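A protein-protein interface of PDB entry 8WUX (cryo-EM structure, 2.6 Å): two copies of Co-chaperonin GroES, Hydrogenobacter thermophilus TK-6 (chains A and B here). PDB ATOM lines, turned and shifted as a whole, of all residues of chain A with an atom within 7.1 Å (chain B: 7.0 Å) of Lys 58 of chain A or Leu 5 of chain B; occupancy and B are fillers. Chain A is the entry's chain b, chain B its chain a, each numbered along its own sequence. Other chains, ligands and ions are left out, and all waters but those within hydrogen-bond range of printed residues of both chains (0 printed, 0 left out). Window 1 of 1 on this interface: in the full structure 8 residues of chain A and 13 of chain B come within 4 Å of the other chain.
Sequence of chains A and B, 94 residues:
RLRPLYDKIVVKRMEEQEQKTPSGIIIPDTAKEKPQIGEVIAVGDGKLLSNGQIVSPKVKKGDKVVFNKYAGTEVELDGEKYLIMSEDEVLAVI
Of chain B, only Leu 5, Tyr 6 and Asp 45 come within 4 Å of Lys 58 of chain A. Of the printed residues of chain B, Val 93 of chain A touches Arg 3 (2.9 Å). Leu 5 of chain B touches one residue of chain A. Of the printed residues of chain A, Asp 45 of chain B touches Lys 58. The nearest residue of chain A that does not touch Leu 5 of chain B is Val 90 of chain A (4.03 Å).
Along chain A the printed residues that touch a printed residue of chain B span positions 58 to 93. Among the printed residues, 6 pairs touch across the chains.
The backbone carbonyl oxygen (O) of Tyr 6 of chain B lies within hydrogen-bond range of the backbone NH (N) of Gly 46 of chain B (2.7 Å). O of Lys 8 of chain B lies within hydrogen-bond range of N of Gly 44 of chain B. The side-chain carboxylate (OD2) of Asp 7 of chain B is in salt-bridge range of the side-chain amino group (NZ) of Lys 8 of chain B, 3.9 Å away. N of Leu 91 of chain A is in hydrogen-bond range of O of Val 66 of chain A (3.2 Å). The backbone carbonyl oxygen of Tyr 6 of chain B sits at hydrogen-bond distance from the backbone NH of Asp 45 of chain B, at 3.0 Å. N of Val 66 of chain A sits at hydrogen-bond distance from O of Ala 92 of chain A (3.1 Å).
Among the printed residues, pairs that only touch across the chains: Ala 92 of chain A with Arg 3 of chain B (3.3 Å), Lys 58 of chain A with Tyr 6 of chain B (3.5 Å), Leu 91 of chain A with Lys 8 of chain B (3.6 Å) and Lys 58 of chain A with Leu 5 of chain B (3.8 Å).
O of Val 93 of chain A sits at hydrogen-bond distance from N of Arg 3 of chain B (2.9 Å). OD1 of Asp 45 of chain B lies within salt-bridge range of NZ of Lys 58 of chain A (3.0 Å).
Position printed for both chains: 43. Of the 6 pairs that touch across the chains among the printed residues, none has its exchanged pair printed and touching as well.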
ATOM      1  N   VAL A  43      17.406 -28.671   5.304  1.00  0.00           N
ATOM      2  CA  VAL A  43      18.240 -29.393   6.256  1.00  0.00           C
ATOM      3  C   VAL A  43      18.900 -30.559   5.537  1.00  0.00           C
ATOM      4  O   VAL A  43      18.397 -31.039   4.516  1.00  0.00           O
ATOM      5  CB  VAL A  43      17.426 -29.892   7.468  1.00  0.00           C
ATOM      6  CG1 VAL A  43      16.812 -28.721   8.215  1.00  0.00           C
ATOM      7  CG2 VAL A  43      16.352 -30.869   7.021  1.00  0.00           C
ATOM      8  N   VAL A  55      21.579 -39.616  12.397  1.00  0.00           N
ATOM      9  CA  VAL A  55      20.517 -39.141  13.277  1.00  0.00           C
ATOM     10  C   VAL A  55      19.791 -38.009  12.562  1.00  0.00           C
ATOM     11  O   VAL A  55      20.428 -37.110  11.998  1.00  0.00           O
ATOM     12  CB  VAL A  55      21.069 -38.687  14.638  1.00  0.00           C
ATOM     13  CG1 VAL A  55      22.270 -37.772  14.453  1.00  0.00           C
ATOM     14  CG2 VAL A  55      19.985 -37.997  15.453  1.00  0.00           C
ATOM     15  N   SER A  56      18.464 -38.064  12.567  1.00  0.00           N
ATOM     16  CA  SER A  56      17.671 -37.048  11.891  1.00  0.00           C
ATOM     17  C   SER A  56      17.904 -35.687  12.540  1.00  0.00           C
ATOM     18  O   SER A  56      17.923 -35.591  13.775  1.00  0.00           O
ATOM     19  CB  SER A  56      16.188 -37.407  11.937  1.00  0.00           C
ATOM     20  OG  SER A  56      15.418 -36.488  11.182  1.00  0.00           O
ATOM     21  N   PRO A  57      18.102 -34.628  11.757  1.00  0.00           N
ATOM     22  CA  PRO A  57      18.312 -33.300  12.346  1.00  0.00           C
ATOM     23  C   PRO A  57      17.117 -32.868  13.182  1.00  0.00           C
ATOM     24  O   PRO A  57      15.963 -33.125  12.833  1.00  0.00           O
ATOM     25  CB  PRO A  57      18.501 -32.395  11.124  1.00  0.00           C
ATOM     26  CG  PRO A  57      18.875 -33.304  10.008  1.00  0.00           C
ATOM     27  CD  PRO A  57      18.237 -34.626  10.291  1.00  0.00           C
ATOM     28  N   LYS A  58      17.402 -32.203  14.299  1.00  0.00           N
ATOM     29  CA  LYS A  58      16.356 -31.706  15.190  1.00  0.00           C
ATOM     30  C   LYS A  58      15.970 -30.270  14.848  1.00  0.00           C
ATOM     31  O   LYS A  58      15.973 -29.380  15.697  1.00  0.00           O
ATOM     32  CB  LYS A  58      16.814 -31.824  16.638  1.00  0.00           C
ATOM     33  CG  LYS A  58      17.036 -33.256  17.092  1.00  0.00           C
ATOM     34  CD  LYS A  58      16.663 -33.439  18.552  1.00  0.00           C
ATOM     35  CE  LYS A  58      16.881 -34.875  18.999  1.00  0.00           C
ATOM     36  NZ  LYS A  58      15.971 -35.252  20.114  1.00  0.00           N
ATOM     37  N   VAL A  59      15.633 -30.043  13.581  1.00  0.00           N
ATOM     38  CA  VAL A  59      15.240 -28.724  13.102  1.00  0.00           C
ATOM     39  C   VAL A  59      14.368 -28.910  11.868  1.00  0.00           C
ATOM     40  O   VAL A  59      14.618 -29.785  11.034  1.00  0.00           O
ATOM     41  CB  VAL A  59      16.477 -27.840  12.807  1.00  0.00           C
ATOM     42  CG1 VAL A  59      17.420 -28.538  11.839  1.00  0.00           C
ATOM     43  CG2 VAL A  59      16.057 -26.480  12.277  1.00  0.00           C
ATOM     44  N   LYS A  60      13.328 -28.085  11.759  1.00  0.00           N
ATOM     45  CA  LYS A  60      12.361 -28.206  10.677  1.00  0.00           C
ATOM     46  C   LYS A  60      12.473 -27.009   9.744  1.00  0.00           C
ATOM     47  O   LYS A  60      13.292 -26.109   9.946  1.00  0.00           O
ATOM     48  CB  LYS A  60      10.921 -28.323  11.203  1.00  0.00           C
ATOM     49  CG  LYS A  60      10.775 -29.080  12.516  1.00  0.00           C
ATOM     50  CD  LYS A  60      11.301 -30.503  12.410  1.00  0.00           C
ATOM     51  CE  LYS A  60      11.503 -31.114  13.785  1.00  0.00           C
ATOM     52  NZ  LYS A  60      12.826 -30.760  14.366  1.00  0.00           N
ATOM     53  N   ASP A  63      11.211 -23.566  11.435  1.00  0.00           N
ATOM     54  CA  ASP A  63      11.799 -23.215  12.717  1.00  0.00           C
ATOM     55  C   ASP A  63      12.573 -21.905  12.626  1.00  0.00           C
ATOM     56  O   ASP A  63      13.135 -21.558  11.582  1.00  0.00           O
ATOM     57  CB  ASP A  63      12.725 -24.329  13.203  1.00  0.00           C
ATOM     58  CG  ASP A  63      12.024 -25.311  14.121  1.00  0.00           C
ATOM     59  OD1 ASP A  63      12.174 -26.532  13.912  1.00  0.00           O
ATOM     60  OD2 ASP A  63      11.323 -24.861  15.051  1.00  0.00           O
ATOM     61  N   VAL A  65      15.774 -20.326  14.106  1.00  0.00           N
ATOM     62  CA  VAL A  65      17.003 -20.767  14.755  1.00  0.00           C
ATOM     63  C   VAL A  65      17.865 -19.551  15.057  1.00  0.00           C
ATOM     64  O   VAL A  65      18.078 -18.697  14.188  1.00  0.00           O
ATOM     65  CB  VAL A  65      17.766 -21.782  13.884  1.00  0.00           C
ATOM     66  CG1 VAL A  65      17.094 -23.143  13.953  1.00  0.00           C
ATOM     67  CG2 VAL A  65      17.841 -21.301  12.444  1.00  0.00           C
ATOM     68  N   VAL A  66      18.347 -19.470  16.293  1.00  0.00           N
ATOM     69  CA  VAL A  66      19.269 -18.428  16.726  1.00  0.00           C
ATOM     70  C   VAL A  66      20.645 -19.057  16.900  1.00  0.00           C
ATOM     71  O   VAL A  66      20.770 -20.155  17.456  1.00  0.00           O
ATOM     72  CB  VAL A  66      18.782 -17.743  18.016  1.00  0.00           C
ATOM     73  CG1 VAL A  66      18.568 -18.762  19.124  1.00  0.00           C
ATOM     74  CG2 VAL A  66      19.767 -16.670  18.455  1.00  0.00           C
ATOM     75  N   GLU A  87      25.022 -28.350  12.773  1.00  0.00           N
ATOM     76  CA  GLU A  87      24.093 -28.574  13.877  1.00  0.00           C
ATOM     77  C   GLU A  87      24.688 -28.191  15.224  1.00  0.00           C
ATOM     78  O   GLU A  87      23.959 -27.765  16.126  1.00  0.00           O
ATOM     79  CB  GLU A  87      23.651 -30.042  13.896  1.00  0.00           C
ATOM     80  CG  GLU A  87      22.235 -30.372  13.363  1.00  0.00           C
ATOM     81  CD  GLU A  87      21.087 -29.486  13.870  1.00  0.00           C
ATOM     82  OE1 GLU A  87      19.926 -29.827  13.560  1.00  0.00           O
ATOM     83  OE2 GLU A  87      21.302 -28.499  14.602  1.00  0.00           O
ATOM     84  N   VAL A  90      24.369 -24.115  16.086  1.00  0.00           N
ATOM     85  CA  VAL A  90      23.110 -23.420  16.325  1.00  0.00           C
ATOM     86  C   VAL A  90      22.726 -23.610  17.787  1.00  0.00           C
ATOM     87  O   VAL A  90      22.481 -24.731  18.244  1.00  0.00           O
ATOM     88  CB  VAL A  90      22.010 -23.913  15.375  1.00  0.00           C
ATOM     89  CG1 VAL A  90      22.050 -25.422  15.234  1.00  0.00           C
ATOM     90  CG2 VAL A  90      20.642 -23.452  15.864  1.00  0.00           C
ATOM     91  N   LEU A  91      22.686 -22.507  18.532  1.00  0.00           N
ATOM     92  CA  LEU A  91      22.568 -22.558  19.984  1.00  0.00           C
ATOM     93  C   LEU A  91      21.169 -22.937  20.463  1.00  0.00           C
ATOM     94  O   LEU A  91      21.039 -23.648  21.465  1.00  0.00           O
ATOM     95  CB  LEU A  91      23.023 -21.218  20.578  1.00  0.00           C
ATOM     96  CG  LEU A  91      22.226 -19.919  20.408  1.00  0.00           C
ATOM     97  CD1 LEU A  91      21.097 -19.778  21.409  1.00  0.00           C
ATOM     98  CD2 LEU A  91      23.165 -18.724  20.494  1.00  0.00           C
ATOM     99  N   ALA A  92      20.121 -22.497  19.770  1.00  0.00           N
ATOM    100  CA  ALA A  92      18.759 -22.832  20.171  1.00  0.00           C
ATOM    101  C   ALA A  92      17.813 -22.544  19.015  1.00  0.00           C
ATOM    102  O   ALA A  92      18.223 -22.081  17.949  1.00  0.00           O
ATOM    103  CB  ALA A  92      18.333 -22.061  21.424  1.00  0.00           C
ATOM    104  N   VAL A  93      16.533 -22.826  19.249  1.00  0.00           N
ATOM    105  CA  VAL A  93      15.484 -22.615  18.260  1.00  0.00           C
ATOM    106  C   VAL A  93      14.324 -21.881  18.921  1.00  0.00           C
ATOM    107  O   VAL A  93      14.052 -22.061  20.113  1.00  0.00           O
ATOM    108  CB  VAL A  93      15.018 -23.950  17.630  1.00  0.00           C
ATOM    109  CG1 VAL A  93      14.251 -24.791  18.637  1.00  0.00           C
ATOM    110  CG2 VAL A  93      14.180 -23.694  16.391  1.00  0.00           C
ATOM    111  N   ARG B   3      13.765 -22.828  22.860  1.00  0.00           N
ATOM    112  CA  ARG B   3      14.033 -24.249  23.029  1.00  0.00           C
ATOM    113  C   ARG B   3      15.504 -24.543  22.783  1.00  0.00           C
ATOM    114  O   ARG B   3      15.985 -24.354  21.657  1.00  0.00           O
ATOM    115  CB  ARG B   3      13.168 -25.073  22.080  1.00  0.00           C
ATOM    116  CG  ARG B   3      11.743 -25.300  22.556  1.00  0.00           C
ATOM    117  CD  ARG B   3      10.883 -25.983  21.489  1.00  0.00           C
ATOM    118  NE  ARG B   3      11.644 -26.797  20.546  1.00  0.00           N
ATOM    119  CZ  ARG B   3      12.249 -27.941  20.844  1.00  0.00           C
ATOM    120  NH1 ARG B   3      12.198 -28.455  22.061  1.00  0.00           N
ATOM    121  NH2 ARG B   3      12.920 -28.586  19.894  1.00  0.00           N
ATOM    122  N   PRO B   4      16.248 -25.000  23.785  1.00  0.00           N
ATOM    123  CA  PRO B   4      17.627 -25.437  23.546  1.00  0.00           C
ATOM    124  C   PRO B   4      17.653 -26.764  22.803  1.00  0.00           C
ATOM    125  O   PRO B   4      16.686 -27.528  22.787  1.00  0.00           O
ATOM    126  CB  PRO B   4      18.205 -25.569  24.955  1.00  0.00           C
ATOM    127  CG  PRO B   4      17.021 -25.884  25.804  1.00  0.00           C
ATOM    128  CD  PRO B   4      15.858 -25.142  25.199  1.00  0.00           C
ATOM    129  N   LEU B   5      18.796 -27.037  22.180  1.00  0.00           N
ATOM    130  CA  LEU B   5      18.979 -28.242  21.384  1.00  0.00           C
ATOM    131  C   LEU B   5      20.009 -29.145  22.046  1.00  0.00           C
ATOM    132  O   LEU B   5      21.056 -28.678  22.504  1.00  0.00           O
ATOM    133  CB  LEU B   5      19.416 -27.906  19.955  1.00  0.00           C
ATOM    134  CG  LEU B   5      18.412 -27.091  19.138  1.00  0.00           C
ATOM    135  CD1 LEU B   5      19.001 -26.710  17.790  1.00  0.00           C
ATOM    136  CD2 LEU B   5      17.113 -27.860  18.964  1.00  0.00           C
ATOM    137  N   TYR B   6      19.703 -30.442  22.078  1.00  0.00           N
ATOM    138  CA  TYR B   6      20.545 -31.457  22.701  1.00  0.00           C
ATOM    139  C   TYR B   6      20.944 -31.088  24.126  1.00  0.00           C
ATOM    140  O   TYR B   6      20.090 -30.993  25.013  1.00  0.00           O
ATOM    141  CB  TYR B   6      21.802 -31.708  21.862  1.00  0.00           C
ATOM    142  CG  TYR B   6      21.532 -32.019  20.407  1.00  0.00           C
ATOM    143  CD1 TYR B   6      20.425 -32.765  20.028  1.00  0.00           C
ATOM    144  CD2 TYR B   6      22.399 -31.582  19.414  1.00  0.00           C
ATOM    145  CE1 TYR B   6      20.182 -33.059  18.702  1.00  0.00           C
ATOM    146  CE2 TYR B   6      22.164 -31.871  18.083  1.00  0.00           C
ATOM    147  CZ  TYR B   6      21.053 -32.609  17.732  1.00  0.00           C
ATOM    148  OH  TYR B   6      20.813 -32.899  16.409  1.00  0.00           O
ATOM    149  N   ASP B   7      22.239 -30.878  24.348  1.00  0.00           N
ATOM    150  CA  ASP B   7      22.777 -30.667  25.686  1.00  0.00           C
ATOM    151  C   ASP B   7      22.789 -29.204  26.111  1.00  0.00           C
ATOM    152  O   ASP B   7      23.282 -28.902  27.202  1.00  0.00           O
ATOM    153  CB  ASP B   7      24.193 -31.244  25.770  1.00  0.00           C
ATOM    154  CG  ASP B   7      25.230 -30.337  25.141  1.00  0.00           C
ATOM    155  OD1 ASP B   7      25.963 -29.660  25.890  1.00  0.00           O
ATOM    156  OD2 ASP B   7      25.312 -30.302  23.895  1.00  0.00           O
ATOM    157  N   LYS B   8      22.271 -28.297  25.289  1.00  0.00           N
ATOM    158  CA  LYS B   8      22.231 -26.892  25.660  1.00  0.00           C
ATOM    159  C   LYS B   8      21.190 -26.652  26.751  1.00  0.00           C
ATOM    160  O   LYS B   8      20.183 -27.356  26.858  1.00  0.00           O
ATOM    161  CB  LYS B   8      21.924 -26.021  24.443  1.00  0.00           C
ATOM    162  CG  LYS B   8      22.963 -26.107  23.339  1.00  0.00           C
ATOM    163  CD  LYS B   8      24.321 -25.628  23.820  1.00  0.00           C
ATOM    164  CE  LYS B   8      25.317 -25.565  22.674  1.00  0.00           C
ATOM    165  NZ  LYS B   8      25.478 -26.884  22.007  1.00  0.00           N
ATOM    166  N   ILE B   9      21.453 -25.638  27.572  1.00  0.00           N
ATOM    167  CA  ILE B   9      20.561 -25.231  28.650  1.00  0.00           C
ATOM    168  C   ILE B   9      20.326 -23.732  28.528  1.00  0.00           C
ATOM    169  O   ILE B   9      21.171 -22.994  28.014  1.00  0.00           O
ATOM    170  CB  ILE B   9      21.139 -25.580  30.041  1.00  0.00           C
ATOM    171  CG1 ILE B   9      21.769 -26.974  30.031  1.00  0.00           C
ATOM    172  CG2 ILE B   9      20.060 -25.512  31.109  1.00  0.00           C
ATOM    173  CD1 ILE B   9      22.797 -27.183  31.119  1.00  0.00           C
ATOM    174  N   VAL B  10      19.170 -23.283  29.006  1.00  0.00           N
ATOM    175  CA  VAL B  10      18.821 -21.867  29.023  1.00  0.00           C
ATOM    176  C   VAL B  10      18.832 -21.401  30.471  1.00  0.00           C
ATOM    177  O   VAL B  10      18.071 -21.911  31.303  1.00  0.00           O
ATOM    178  CB  VAL B  10      17.455 -21.616  28.367  1.00  0.00           C
ATOM    179  CG1 VAL B  10      17.225 -20.126  28.175  1.00  0.00           C
ATOM    180  CG2 VAL B  10      17.369 -22.352  27.042  1.00  0.00           C
ATOM    181  N   VAL B  43      15.473 -26.692  29.394  1.00  0.00           N
ATOM    182  CA  VAL B  43      16.417 -27.801  29.359  1.00  0.00           C
ATOM    183  C   VAL B  43      16.241 -28.552  28.047  1.00  0.00           C
ATOM    184  O   VAL B  43      15.115 -28.870  27.648  1.00  0.00           O
ATOM    185  CB  VAL B  43      16.223 -28.750  30.560  1.00  0.00           C
ATOM    186  CG1 VAL B  43      17.121 -29.967  30.428  1.00  0.00           C
ATOM    187  CG2 VAL B  43      16.502 -28.019  31.862  1.00  0.00           C
ATOM    188  N   GLY B  44      17.355 -28.838  27.379  1.00  0.00           N
ATOM    189  CA  GLY B  44      17.333 -29.555  26.125  1.00  0.00           C
ATOM    190  C   GLY B  44      17.155 -31.050  26.320  1.00  0.00           C
ATOM    191  O   GLY B  44      17.001 -31.559  27.430  1.00  0.00           O
ATOM    192  N   ASP B  45      17.175 -31.765  25.192  1.00  0.00           N
ATOM    193  CA  ASP B  45      16.984 -33.210  25.214  1.00  0.00           C
ATOM    194  C   ASP B  45      18.118 -33.934  25.930  1.00  0.00           C
ATOM    195  O   ASP B  45      17.863 -34.894  26.665  1.00  0.00           O
ATOM    196  CB  ASP B  45      16.836 -33.740  23.788  1.00  0.00           C
ATOM    197  CG  ASP B  45      16.006 -32.825  22.913  1.00  0.00           C
ATOM    198  OD1 ASP B  45      16.263 -32.770  21.692  1.00  0.00           O
ATOM    199  OD2 ASP B  45      15.092 -32.159  23.445  1.00  0.00           O
ATOM    200  N   GLY B  46      19.356 -33.504  25.730  1.00  0.00           N
ATOM    201  CA  GLY B  46      20.497 -34.093  26.400  1.00  0.00           C
ATOM    202  C   GLY B  46      21.668 -34.302  25.460  1.00  0.00           C
ATOM    203  O   GLY B  46      21.576 -34.126  24.246  1.00  0.00           O
ATOM    204  N   LEU B  48      24.470 -35.959  23.182  1.00  0.00           N
ATOM    205  CA  LEU B  48      24.461 -37.030  22.192  1.00  0.00           C
ATOM    206  C   LEU B  48      25.697 -37.899  22.388  1.00  0.00           C
ATOM    207  O   LEU B  48      26.821 -37.462  22.123  1.00  0.00           O
ATOM    208  CB  LEU B  48      24.419 -36.456  20.779  1.00  0.00           C
ATOM    209  CG  LEU B  48      23.051 -36.436  20.101  1.00  0.00           C
ATOM    210  CD1 LEU B  48      22.078 -35.612  20.920  1.00  0.00           C
ATOM    211  CD2 LEU B  48      23.161 -35.894  18.685  1.00  0.00           C
ATOM    212  N   ILE B  54      20.874 -40.994  23.980  1.00  0.00           N
ATOM    213  CA  ILE B  54      20.572 -39.697  24.571  1.00  0.00           C
ATOM    214  C   ILE B  54      20.520 -39.860  26.083  1.00  0.00           C
ATOM    215  O   ILE B  54      19.833 -40.752  26.591  1.00  0.00           O
ATOM    216  CB  ILE B  54      19.241 -39.124  24.048  1.00  0.00           C
ATOM    217  CG1 ILE B  54      19.132 -39.319  22.535  1.00  0.00           C
ATOM    218  CG2 ILE B  54      19.119 -37.652  24.408  1.00  0.00           C
ATOM    219  CD1 ILE B  54      20.158 -38.551  21.745  1.00  0.00           C
